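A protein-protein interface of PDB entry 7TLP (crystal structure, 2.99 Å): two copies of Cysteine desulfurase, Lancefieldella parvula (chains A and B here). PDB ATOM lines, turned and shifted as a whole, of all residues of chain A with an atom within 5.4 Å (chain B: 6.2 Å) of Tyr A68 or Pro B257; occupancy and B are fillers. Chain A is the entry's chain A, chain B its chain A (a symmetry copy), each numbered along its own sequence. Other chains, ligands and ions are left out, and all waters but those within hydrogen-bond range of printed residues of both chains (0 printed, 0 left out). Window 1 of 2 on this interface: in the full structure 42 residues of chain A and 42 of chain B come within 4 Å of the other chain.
The side-chain amide nitrogen of Asn A72 lies close to the side-chain amide nitrogen of Gln B55 (3.0 Å).
The side-chain amide oxygen (OD1) of Asn A72 is in hydrogen-bond range of the guanidinium group (NH2) of Arg B56, at 3.0 Å.
The side-chain amide nitrogen of Gln A64 sits close to the side-chain amide nitrogen of Gln B64, 2.3 Å away.
The backbone NH of Met B258 sits close to the side-chain hydroxyl of Tyr A68.
The side-chain carboxylate (OD1) of Asp A306 sits close to the backbone carbonyl oxygen (O) of Met B258, 3.4 Å away.
OD2 of Asp B306 lies close to OD2 of Asp A306, at 3.1 Å.
The side-chain hydroxyl of Thr A70 sits at hydrogen-bond distance from the backbone carbonyl oxygen of Arg A66 (3.2 Å).
The backbone carbonyl oxygen of Phe A67 sits at hydrogen-bond distance from the backbone NH of Asn A72 (3.3 Å).
The backbone carbonyl oxygen of Gln B55 sits at hydrogen-bond distance from the side-chain sulfur of Cys B255 (3.5 Å).
NH1 of Arg B56 lies within hydrogen-bond range of O of His B252 (2.9 Å).
The guanidinium group (NH2) of Arg B56 sits close to the side-chain sulfur (SD) of Met B258 (3.8 Å).
OD1 of Asp B306 sits at hydrogen-bond distance from N of Gly B309, 3.3 Å away.
Among the printed residues, pairs that only touch across the chains: Ala A308 with Met B258, Tyr A68 with Arg B56, Tyr A68 with Pro B257, Phe A67 with Met B258, Glu A69 with Ile B38, Thr A70 with Ile B38, Ser A65 with Ile B61, Met A71 with Ile B38, Tyr A68 with Ile B61 and Asp A306 with Gly B259.
Of the printed residues of chain B, Ser A65 touches Ile B61.
Tyr A68 touches just these residues of chain B: Arg B56, Ile B61, Pro B257 and Met B258.
Printed residues of chain B within 4 Å of Asn A72: Gln B55 and Arg B56.
Of the printed residues of chain B, Ala A308 touches Met B258.
Of the printed residues of chain A, Gln B55 touches Asn A72 (3.0 Å).
Of the printed residues of chain A, Gln B64 touches Gln A64.
Of chain A, only Tyr A68 comes within 4 Å of Pro B257.
The nearest printed residue of chain B that does not touch Tyr A68 is Gln B64 (4.3 Å).
The nearest printed residue of chain A that does not touch Pro B257 is Asp A306 (5.7 Å).
Printed residues of chain B that touch a printed residue of chain A: Ile B38, Gln B55, Arg B56, Ile B61, Gln B64, Pro B257, Met B258, Gly B259 and Asp B306.
Hydrophobic or aromatic side chains of chain B that line the printed part of chain A: Ile B38, Ile B61, Pro B257 and Met B258.
Of the 11 printed residues of chain A, 10 touch a printed residue of chain B.
Printed residues of chain A that touch a printed residue of chain B: Gln A64, Ser A65, Phe A67, Tyr A68, Glu A69, Thr A70, Met A71, Asn A72, Asp A306 and Ala A308.
Hydrophobic or aromatic side chains of chain A that line the printed part of chain B: Phe A67 and Tyr A68.
Among the printed residues, no Asp or Glu carboxylate lies within 4 Å of a Lys or Arg side-chain nitrogen of the other chain.
Gln A64 touches its own counterpart, Gln B64.
Asp A306 touches its own counterpart, Asp B306.
Of the 16 pairs that touch across the chains among the printed residues, 2 have their exchanged pair printed and touching as well.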
ATOM      1  N   GLN A  64     -26.354  -3.241 -17.281  1.00  0.00           N
ATOM      2  CA  GLN A  64     -25.536  -2.888 -18.420  1.00  0.00           C
ATOM      3  C   GLN A  64     -26.280  -3.160 -19.722  1.00  0.00           C
ATOM      4  O   GLN A  64     -26.189  -2.382 -20.688  1.00  0.00           O
ATOM      5  CB  GLN A  64     -24.240  -3.652 -18.300  1.00  0.00           C
ATOM      6  CG  GLN A  64     -23.296  -3.454 -19.378  1.00  0.00           C
ATOM      7  CD  GLN A  64     -22.162  -4.386 -19.215  1.00  0.00           C
ATOM      8  OE1 GLN A  64     -21.484  -4.416 -18.188  1.00  0.00           O
ATOM      9  NE2 GLN A  64     -22.006  -5.228 -20.153  1.00  0.00           N
ATOM     10  N   SER A  65     -27.044  -4.252 -19.744  1.00  0.00           N
ATOM     11  CA  SER A  65     -27.953  -4.493 -20.849  1.00  0.00           C
ATOM     12  C   SER A  65     -28.920  -3.324 -20.980  1.00  0.00           C
ATOM     13  O   SER A  65     -29.079  -2.748 -22.063  1.00  0.00           O
ATOM     14  CB  SER A  65     -28.681  -5.825 -20.631  1.00  0.00           C
ATOM     15  N   ARG A  66     -29.531  -2.928 -19.858  1.00  0.00           N
ATOM     16  CA  ARG A  66     -30.366  -1.733 -19.770  1.00  0.00           C
ATOM     17  C   ARG A  66     -29.742  -0.545 -20.485  1.00  0.00           C
ATOM     18  O   ARG A  66     -30.354   0.037 -21.375  1.00  0.00           O
ATOM     19  CB  ARG A  66     -30.618  -1.390 -18.293  1.00  0.00           C
ATOM     20  CG  ARG A  66     -31.479  -0.162 -18.029  1.00  0.00           C
ATOM     21  CD  ARG A  66     -32.837  -0.339 -18.612  1.00  0.00           C
ATOM     22  NE  ARG A  66     -33.234  -1.731 -18.457  1.00  0.00           N
ATOM     23  CZ  ARG A  66     -33.724  -2.289 -17.350  1.00  0.00           C
ATOM     24  NH1 ARG A  66     -33.954  -1.569 -16.255  1.00  0.00           N
ATOM     25  NH2 ARG A  66     -34.035  -3.584 -17.365  1.00  0.00           N
ATOM     26  N   PHE A  67     -28.520  -0.174 -20.105  1.00  0.00           N
ATOM     27  CA  PHE A  67     -27.874   0.981 -20.710  1.00  0.00           C
ATOM     28  C   PHE A  67     -28.012   0.954 -22.217  1.00  0.00           C
ATOM     29  O   PHE A  67     -28.477   1.917 -22.822  1.00  0.00           O
ATOM     30  CB  PHE A  67     -26.394   1.015 -20.338  1.00  0.00           C
ATOM     31  CG  PHE A  67     -25.660   2.256 -20.840  1.00  0.00           C
ATOM     32  CD1 PHE A  67     -25.410   3.321 -19.978  1.00  0.00           C
ATOM     33  CD2 PHE A  67     -25.247   2.353 -22.180  1.00  0.00           C
ATOM     34  CE1 PHE A  67     -24.764   4.427 -20.426  1.00  0.00           C
ATOM     35  CE2 PHE A  67     -24.609   3.473 -22.647  1.00  0.00           C
ATOM     36  CZ  PHE A  67     -24.364   4.514 -21.779  1.00  0.00           C
ATOM     37  N   TYR A  68     -27.600  -0.158 -22.831  1.00  0.00           N
ATOM     38  CA  TYR A  68     -27.542  -0.284 -24.285  1.00  0.00           C
ATOM     39  C   TYR A  68     -28.923  -0.230 -24.907  1.00  0.00           C
ATOM     40  O   TYR A  68     -29.070   0.199 -26.059  1.00  0.00           O
ATOM     41  CB  TYR A  68     -26.861  -1.605 -24.674  1.00  0.00           C
ATOM     42  CG  TYR A  68     -25.375  -1.504 -24.725  1.00  0.00           C
ATOM     43  CD1 TYR A  68     -24.785  -0.403 -25.315  1.00  0.00           C
ATOM     44  CD2 TYR A  68     -24.561  -2.478 -24.177  1.00  0.00           C
ATOM     45  CE1 TYR A  68     -23.415  -0.261 -25.381  1.00  0.00           C
ATOM     46  CE2 TYR A  68     -23.167  -2.354 -24.234  1.00  0.00           C
ATOM     47  CZ  TYR A  68     -22.605  -1.226 -24.846  1.00  0.00           C
ATOM     48  OH  TYR A  68     -21.255  -1.026 -24.958  1.00  0.00           O
ATOM     49  N   GLU A  69     -29.936  -0.665 -24.166  1.00  0.00           N
ATOM     50  CA  GLU A  69     -31.283  -0.731 -24.691  1.00  0.00           C
ATOM     51  C   GLU A  69     -32.067   0.560 -24.483  1.00  0.00           C
ATOM     52  O   GLU A  69     -33.055   0.789 -25.189  1.00  0.00           O
ATOM     53  CB  GLU A  69     -32.017  -1.925 -24.068  1.00  0.00           C
ATOM     54  N   THR A  70     -31.639   1.445 -23.595  1.00  0.00           N
ATOM     55  CA  THR A  70     -32.357   2.703 -23.438  1.00  0.00           C
ATOM     56  C   THR A  70     -31.545   3.976 -23.706  1.00  0.00           C
ATOM     57  O   THR A  70     -32.152   5.009 -23.971  1.00  0.00           O
ATOM     58  CB  THR A  70     -32.989   2.801 -22.033  1.00  0.00           C
ATOM     59  OG1 THR A  70     -31.983   2.779 -21.021  1.00  0.00           O
ATOM     60  CG2 THR A  70     -33.937   1.656 -21.798  1.00  0.00           C
ATOM     61  N   MET A  71     -30.217   3.947 -23.668  1.00  0.00           N
ATOM     62  CA  MET A  71     -29.477   5.204 -23.761  1.00  0.00           C
ATOM     63  C   MET A  71     -28.441   5.214 -24.882  1.00  0.00           C
ATOM     64  O   MET A  71     -28.519   6.036 -25.798  1.00  0.00           O
ATOM     65  CB  MET A  71     -28.815   5.514 -22.415  1.00  0.00           C
ATOM     66  CG  MET A  71     -29.804   5.980 -21.350  1.00  0.00           C
ATOM     67  SD  MET A  71     -29.131   6.095 -19.653  1.00  0.00           S
ATOM     68  CE  MET A  71     -28.488   4.446 -19.372  1.00  0.00           C
ATOM     69  N   ASN A  72     -27.473   4.315 -24.810  1.00  0.00           N
ATOM     70  CA  ASN A  72     -26.339   4.231 -25.733  1.00  0.00           C
ATOM     71  C   ASN A  72     -25.590   5.570 -25.805  1.00  0.00           C
ATOM     72  O   ASN A  72     -25.498   6.181 -26.866  1.00  0.00           O
ATOM     73  CB  ASN A  72     -26.809   3.791 -27.123  1.00  0.00           C
ATOM     74  CG  ASN A  72     -25.852   2.815 -27.772  1.00  0.00           C
ATOM     75  OD1 ASN A  72     -24.911   2.338 -27.140  1.00  0.00           O
ATOM     76  ND2 ASN A  72     -26.107   2.482 -29.020  1.00  0.00           N
ATOM     77  N   ASP A 306     -16.373   2.748 -22.320  1.00  0.00           N
ATOM     78  CA  ASP A 306     -17.365   1.709 -22.076  1.00  0.00           C
ATOM     79  C   ASP A 306     -18.461   2.248 -21.151  1.00  0.00           C
ATOM     80  O   ASP A 306     -18.602   1.859 -19.988  1.00  0.00           O
ATOM     81  CB  ASP A 306     -16.667   0.498 -21.489  1.00  0.00           C
ATOM     82  CG  ASP A 306     -17.450  -0.785 -21.639  1.00  0.00           C
ATOM     83  OD1 ASP A 306     -18.646  -0.689 -22.090  1.00  0.00           O
ATOM     84  OD2 ASP A 306     -16.824  -1.868 -21.279  1.00  0.00           O
ATOM     85  N   ALA A 308     -21.696   1.782 -21.031  1.00  0.00           N
ATOM     86  CA  ALA A 308     -22.559   0.748 -20.446  1.00  0.00           C
ATOM     87  C   ALA A 308     -21.859  -0.003 -19.318  1.00  0.00           C
ATOM     88  O   ALA A 308     -22.505  -0.392 -18.343  1.00  0.00           O
ATOM     89  CB  ALA A 308     -23.048  -0.236 -21.512  1.00  0.00           C
ATOM     90  N   PRO B  37     -33.575  -2.674 -29.976  1.00  0.00           N
ATOM     91  CA  PRO B  37     -34.552  -2.352 -28.921  1.00  0.00           C
ATOM     92  C   PRO B  37     -34.805  -0.875 -28.761  1.00  0.00           C
ATOM     93  O   PRO B  37     -35.955  -0.471 -28.578  1.00  0.00           O
ATOM     94  CB  PRO B  37     -33.913  -2.951 -27.664  1.00  0.00           C
ATOM     95  CG  PRO B  37     -33.015  -4.014 -28.194  1.00  0.00           C
ATOM     96  CD  PRO B  37     -32.441  -3.439 -29.456  1.00  0.00           C
ATOM     97  N   ILE B  38     -33.755  -0.062 -28.854  1.00  0.00           N
ATOM     98  CA  ILE B  38     -33.859   1.373 -28.611  1.00  0.00           C
ATOM     99  C   ILE B  38     -34.627   2.036 -29.745  1.00  0.00           C
ATOM    100  O   ILE B  38     -35.408   2.965 -29.522  1.00  0.00           O
ATOM    101  CB  ILE B  38     -32.443   1.950 -28.467  1.00  0.00           C
ATOM    102  CG1 ILE B  38     -32.417   3.381 -27.988  1.00  0.00           C
ATOM    103  CG2 ILE B  38     -31.821   1.957 -29.848  1.00  0.00           C
ATOM    104  CD1 ILE B  38     -31.089   3.745 -27.362  1.00  0.00           C
ATOM    105  N   GLN B  55     -26.331   1.771 -33.139  1.00  0.00           N
ATOM    106  CA  GLN B  55     -27.179   1.137 -32.150  1.00  0.00           C
ATOM    107  C   GLN B  55     -26.902  -0.346 -32.055  1.00  0.00           C
ATOM    108  O   GLN B  55     -26.312  -0.953 -32.948  1.00  0.00           O
ATOM    109  CB  GLN B  55     -28.646   1.302 -32.428  1.00  0.00           C
ATOM    110  CG  GLN B  55     -29.095   2.672 -32.361  1.00  0.00           C
ATOM    111  CD  GLN B  55     -28.700   3.354 -31.038  1.00  0.00           C
ATOM    112  OE1 GLN B  55     -27.973   4.337 -31.094  1.00  0.00           O
ATOM    113  NE2 GLN B  55     -29.003   2.728 -29.864  1.00  0.00           N
ATOM    114  N   ARG B  56     -27.363  -0.933 -30.957  1.00  0.00           N
ATOM    115  CA  ARG B  56     -27.028  -2.326 -30.701  1.00  0.00           C
ATOM    116  C   ARG B  56     -28.204  -3.202 -31.048  1.00  0.00           C
ATOM    117  O   ARG B  56     -29.343  -2.854 -30.689  1.00  0.00           O
ATOM    118  CB  ARG B  56     -26.640  -2.546 -29.244  1.00  0.00           C
ATOM    119  CG  ARG B  56     -25.862  -1.410 -28.632  1.00  0.00           C
ATOM    120  CD  ARG B  56     -24.422  -1.462 -29.016  1.00  0.00           C
ATOM    121  NE  ARG B  56     -23.845  -0.183 -28.645  1.00  0.00           N
ATOM    122  CZ  ARG B  56     -23.044   0.549 -29.409  1.00  0.00           C
ATOM    123  NH1 ARG B  56     -22.692   0.140 -30.618  1.00  0.00           N
ATOM    124  NH2 ARG B  56     -22.608   1.708 -28.954  1.00  0.00           N
ATOM    125  N   VAL B  60     -26.885  -8.795 -29.763  1.00  0.00           N
ATOM    126  CA  VAL B  60     -25.592  -8.402 -29.197  1.00  0.00           C
ATOM    127  C   VAL B  60     -25.736  -8.019 -27.729  1.00  0.00           C
ATOM    128  O   VAL B  60     -24.858  -8.319 -26.916  1.00  0.00           O
ATOM    129  CB  VAL B  60     -24.964  -7.260 -30.021  1.00  0.00           C
ATOM    130  CG1 VAL B  60     -23.618  -6.827 -29.443  1.00  0.00           C
ATOM    131  CG2 VAL B  60     -24.798  -7.690 -31.446  1.00  0.00           C
ATOM    132  N   ILE B  61     -26.839  -7.352 -27.365  1.00  0.00           N
ATOM    133  CA  ILE B  61     -27.096  -7.049 -25.960  1.00  0.00           C
ATOM    134  C   ILE B  61     -27.210  -8.349 -25.164  1.00  0.00           C
ATOM    135  O   ILE B  61     -26.482  -8.562 -24.185  1.00  0.00           O
ATOM    136  CB  ILE B  61     -28.347  -6.163 -25.804  1.00  0.00           C
ATOM    137  CG1 ILE B  61     -28.132  -4.799 -26.488  1.00  0.00           C
ATOM    138  CG2 ILE B  61     -28.653  -5.916 -24.329  1.00  0.00           C
ATOM    139  CD1 ILE B  61     -29.434  -3.957 -26.753  1.00  0.00           C
ATOM    140  N   GLN B  64     -23.994 -10.595 -24.607  1.00  0.00           N
ATOM    141  CA  GLN B  64     -23.000 -10.199 -23.636  1.00  0.00           C
ATOM    142  C   GLN B  64     -23.504 -10.442 -22.218  1.00  0.00           C
ATOM    143  O   GLN B  64     -22.744 -10.869 -21.331  1.00  0.00           O
ATOM    144  CB  GLN B  64     -22.651  -8.755 -23.908  1.00  0.00           C
ATOM    145  CG  GLN B  64     -21.686  -8.166 -23.007  1.00  0.00           C
ATOM    146  CD  GLN B  64     -21.576  -6.719 -23.285  1.00  0.00           C
ATOM    147  OE1 GLN B  64     -21.285  -6.289 -24.402  1.00  0.00           O
ATOM    148  NE2 GLN B  64     -21.909  -5.951 -22.330  1.00  0.00           N
ATOM    149  N   SER B 250     -13.160   0.291 -34.187  1.00  0.00           N
ATOM    150  CA  SER B 250     -13.878   0.027 -32.950  1.00  0.00           C
ATOM    151  C   SER B 250     -15.081  -0.863 -33.227  1.00  0.00           C
ATOM    152  O   SER B 250     -15.530  -1.007 -34.361  1.00  0.00           O
ATOM    153  CB  SER B 250     -14.313   1.327 -32.245  1.00  0.00           C
ATOM    154  OG  SER B 250     -13.209   2.005 -31.646  1.00  0.00           O
ATOM    155  N   ALA B 251     -15.586  -1.503 -32.189  1.00  0.00           N
ATOM    156  CA  ALA B 251     -16.716  -2.377 -32.425  1.00  0.00           C
ATOM    157  C   ALA B 251     -18.031  -1.649 -32.293  1.00  0.00           C
ATOM    158  O   ALA B 251     -19.045  -2.146 -32.775  1.00  0.00           O
ATOM    159  CB  ALA B 251     -16.704  -3.565 -31.467  1.00  0.00           C
ATOM    160  N   HIS B 252     -18.045  -0.490 -31.661  1.00  0.00           N
ATOM    161  CA  HIS B 252     -19.326   0.138 -31.409  1.00  0.00           C
ATOM    162  C   HIS B 252     -19.855   0.921 -32.595  1.00  0.00           C
ATOM    163  O   HIS B 252     -20.939   1.503 -32.467  1.00  0.00           O
ATOM    164  CB  HIS B 252     -19.241   1.044 -30.183  1.00  0.00           C
ATOM    165  CG  HIS B 252     -18.237   2.136 -30.313  1.00  0.00           C
ATOM    166  ND1 HIS B 252     -18.578   3.401 -30.726  1.00  0.00           N
ATOM    167  CD2 HIS B 252     -16.902   2.156 -30.100  1.00  0.00           C
ATOM    168  CE1 HIS B 252     -17.495   4.153 -30.773  1.00  0.00           C
ATOM    169  NE2 HIS B 252     -16.466   3.424 -30.393  1.00  0.00           N
ATOM    170  N   MET B 254     -19.781  -0.746 -35.760  1.00  0.00           N
ATOM    171  CA  MET B 254     -20.454  -1.922 -36.281  1.00  0.00           C
ATOM    172  C   MET B 254     -21.168  -2.689 -35.191  1.00  0.00           C
ATOM    173  O   MET B 254     -20.803  -3.809 -34.874  1.00  0.00           O
ATOM    174  CB  MET B 254     -19.463  -2.821 -36.980  1.00  0.00           C
ATOM    175  CG  MET B 254     -18.225  -3.186 -36.191  1.00  0.00           C
ATOM    176  SD  MET B 254     -17.194  -4.235 -37.286  1.00  0.00           S
ATOM    177  CE  MET B 254     -16.978  -3.211 -38.783  1.00  0.00           C
ATOM    178  N   CYS B 255     -22.171  -2.047 -34.615  1.00  0.00           N
ATOM    179  CA  CYS B 255     -23.185  -2.731 -33.829  1.00  0.00           C
ATOM    180  C   CYS B 255     -22.657  -3.530 -32.643  1.00  0.00           C
ATOM    181  O   CYS B 255     -23.432  -4.279 -32.036  1.00  0.00           O
ATOM    182  CB  CYS B 255     -23.998  -3.678 -34.710  1.00  0.00           C
ATOM    183  SG  CYS B 255     -25.281  -2.926 -35.626  1.00  0.00           S
ATOM    184  N   GLY B 256     -21.375  -3.423 -32.320  1.00  0.00           N
ATOM    185  CA  GLY B 256     -20.820  -4.171 -31.229  1.00  0.00           C
ATOM    186  C   GLY B 256     -20.833  -3.356 -29.957  1.00  0.00           C
ATOM    187  O   GLY B 256     -21.289  -2.207 -29.920  1.00  0.00           O
ATOM    188  N   PRO B 257     -20.333  -3.943 -28.882  1.00  0.00           N
ATOM    189  CA  PRO B 257     -20.383  -3.254 -27.591  1.00  0.00           C
ATOM    190  C   PRO B 257     -19.346  -2.139 -27.539  1.00  0.00           C
ATOM    191  O   PRO B 257     -18.358  -2.118 -28.290  1.00  0.00           O
ATOM    192  CB  PRO B 257     -20.077  -4.371 -26.581  1.00  0.00           C
ATOM    193  CG  PRO B 257     -19.190  -5.326 -27.334  1.00  0.00           C
ATOM    194  CD  PRO B 257     -19.576  -5.209 -28.817  1.00  0.00           C
ATOM    195  N   MET B 258     -19.590  -1.181 -26.650  1.00  0.00           N
ATOM    196  CA  MET B 258     -18.513  -0.265 -26.338  1.00  0.00           C
ATOM    197  C   MET B 258     -17.452  -1.001 -25.503  1.00  0.00           C
ATOM    198  O   MET B 258     -17.668  -2.103 -24.996  1.00  0.00           O
ATOM    199  CB  MET B 258     -19.072   1.002 -25.671  1.00  0.00           C
ATOM    200  CG  MET B 258     -20.385   1.545 -26.340  1.00  0.00           C
ATOM    201  SD  MET B 258     -21.114   3.164 -25.801  1.00  0.00           S
ATOM    202  CE  MET B 258     -21.701   2.573 -24.216  1.00  0.00           C
ATOM    203  N   GLY B 259     -16.260  -0.423 -25.448  1.00  0.00           N
ATOM    204  CA  GLY B 259     -15.148  -1.070 -24.791  1.00  0.00           C
ATOM    205  C   GLY B 259     -14.265  -1.930 -25.670  1.00  0.00           C
ATOM    206  O   GLY B 259     -13.234  -2.392 -25.198  1.00  0.00           O
ATOM    207  N   ILE B 260     -14.608  -2.154 -26.928  1.00  0.00           N
ATOM    208  CA  ILE B 260     -13.833  -3.061 -27.773  1.00  0.00           C
ATOM    209  C   ILE B 260     -13.352  -2.316 -29.010  1.00  0.00           C
ATOM    210  O   ILE B 260     -14.162  -1.907 -29.848  1.00  0.00           O
ATOM    211  CB  ILE B 260     -14.632  -4.308 -28.181  1.00  0.00           C
ATOM    212  CG1 ILE B 260     -15.077  -5.111 -26.945  1.00  0.00           C
ATOM    213  CG2 ILE B 260     -13.810  -5.140 -29.160  1.00  0.00           C
ATOM    214  CD1 ILE B 260     -13.929  -5.568 -25.982  1.00  0.00           C
ATOM    215  N   ASP B 306     -12.060  -7.533 -21.596  1.00  0.00           N
ATOM    216  CA  ASP B 306     -13.517  -7.505 -21.613  1.00  0.00           C
ATOM    217  C   ASP B 306     -14.047  -8.716 -22.388  1.00  0.00           C
ATOM    218  O   ASP B 306     -14.601  -8.614 -23.487  1.00  0.00           O
ATOM    219  CB  ASP B 306     -13.971  -6.194 -22.223  1.00  0.00           C
ATOM    220  CG  ASP B 306     -15.392  -5.820 -21.870  1.00  0.00           C
ATOM    221  OD1 ASP B 306     -16.087  -6.697 -21.243  1.00  0.00           O
ATOM    222  OD2 ASP B 306     -15.771  -4.636 -22.252  1.00  0.00           O
ATOM    223  N   ALA B 308     -16.645 -10.659 -21.968  1.00  0.00           N
ATOM    224  CA  ALA B 308     -18.062 -10.566 -22.343  1.00  0.00           C
ATOM    225  C   ALA B 308     -18.278  -9.616 -23.516  1.00  0.00           C
ATOM    226  O   ALA B 308     -19.153  -9.855 -24.349  1.00  0.00           O
ATOM    227  CB  ALA B 308     -18.925 -10.141 -21.152  1.00  0.00           C
ATOM    228  N   GLY B 309     -17.485  -8.553 -23.598  1.00  0.00           N
ATOM    229  CA  GLY B 309     -17.528  -7.652 -24.723  1.00  0.00           C
ATOM    230  C   GLY B 309     -16.879  -8.195 -25.981  1.00  0.00           C
ATOM    231  O   GLY B 309     -17.419  -7.985 -27.076  1.00  0.00           O
ATOM    232  N   ILE B 310     -15.723  -8.865 -25.862  1.00  0.00           N
ATOM    233  CA  ILE B 310     -15.185  -9.584 -27.010  1.00  0.00           C
ATOM    234  C   ILE B 310     -16.183 -10.627 -27.496  1.00  0.00           C
ATOM    235  O   ILE B 310     -16.292 -10.894 -28.699  1.00  0.00           O
ATOM    236  CB  ILE B 310     -13.822 -10.224 -26.677  1.00  0.00           C
ATOM    237  CG1 ILE B 310     -12.768  -9.189 -26.279  1.00  0.00           C
ATOM    238  CG2 ILE B 310     -13.321 -11.124 -27.808  1.00  0.00           C
ATOM    239  CD1 ILE B 310     -11.730  -9.732 -25.231  1.00  0.00           C
ATOM    240  N   ALA B 312     -19.534 -10.427 -27.305  1.00  0.00           N
ATOM    241  CA  ALA B 312     -20.599  -9.732 -28.009  1.00  0.00           C
ATOM    242  C   ALA B 312     -20.090  -9.176 -29.318  1.00  0.00           C
ATOM    243  O   ALA B 312     -20.850  -9.079 -30.288  1.00  0.00           O
ATOM    244  CB  ALA B 312     -21.173  -8.628 -27.130  1.00  0.00           C
ATOM    245  N   THR B 313     -18.805  -8.818 -29.359  1.00  0.00           N
ATOM    246  CA  THR B 313     -18.226  -8.354 -30.607  1.00  0.00           C
ATOM    247  C   THR B 313     -18.316  -9.445 -31.658  1.00  0.00           C
ATOM    248  O   THR B 313     -18.610  -9.168 -32.839  1.00  0.00           O
ATOM    249  CB  THR B 313     -16.790  -7.914 -30.382  1.00  0.00           C
ATOM    250  OG1 THR B 313     -16.805  -6.875 -29.410  1.00  0.00           O
ATOM    251  CG2 THR B 313     -16.192  -7.379 -31.679  1.00  0.00           C
ATOM    252  N   GLY B 314     -18.107 -10.695 -31.228  1.00  0.00           N
ATOM    253  CA  GLY B 314     -18.375 -11.825 -32.096  1.00  0.00           C
ATOM    254  C   GLY B 314     -19.835 -11.913 -32.514  1.00  0.00           C
ATOM    255  O   GLY B 314     -20.142 -12.102 -33.694  1.00  0.00           O
ATOM    256  N   ALA B 316     -21.888  -9.588 -32.870  1.00  0.00           N
ATOM    257  CA  ALA B 316     -22.160  -8.515 -33.823  1.00  0.00           C
ATOM    258  C   ALA B 316     -21.605  -8.857 -35.193  1.00  0.00           C
ATOM    259  O   ALA B 316     -22.292  -8.686 -36.201  1.00  0.00           O
ATOM    260  CB  ALA B 316     -21.594  -7.186 -33.327  1.00  0.00           C
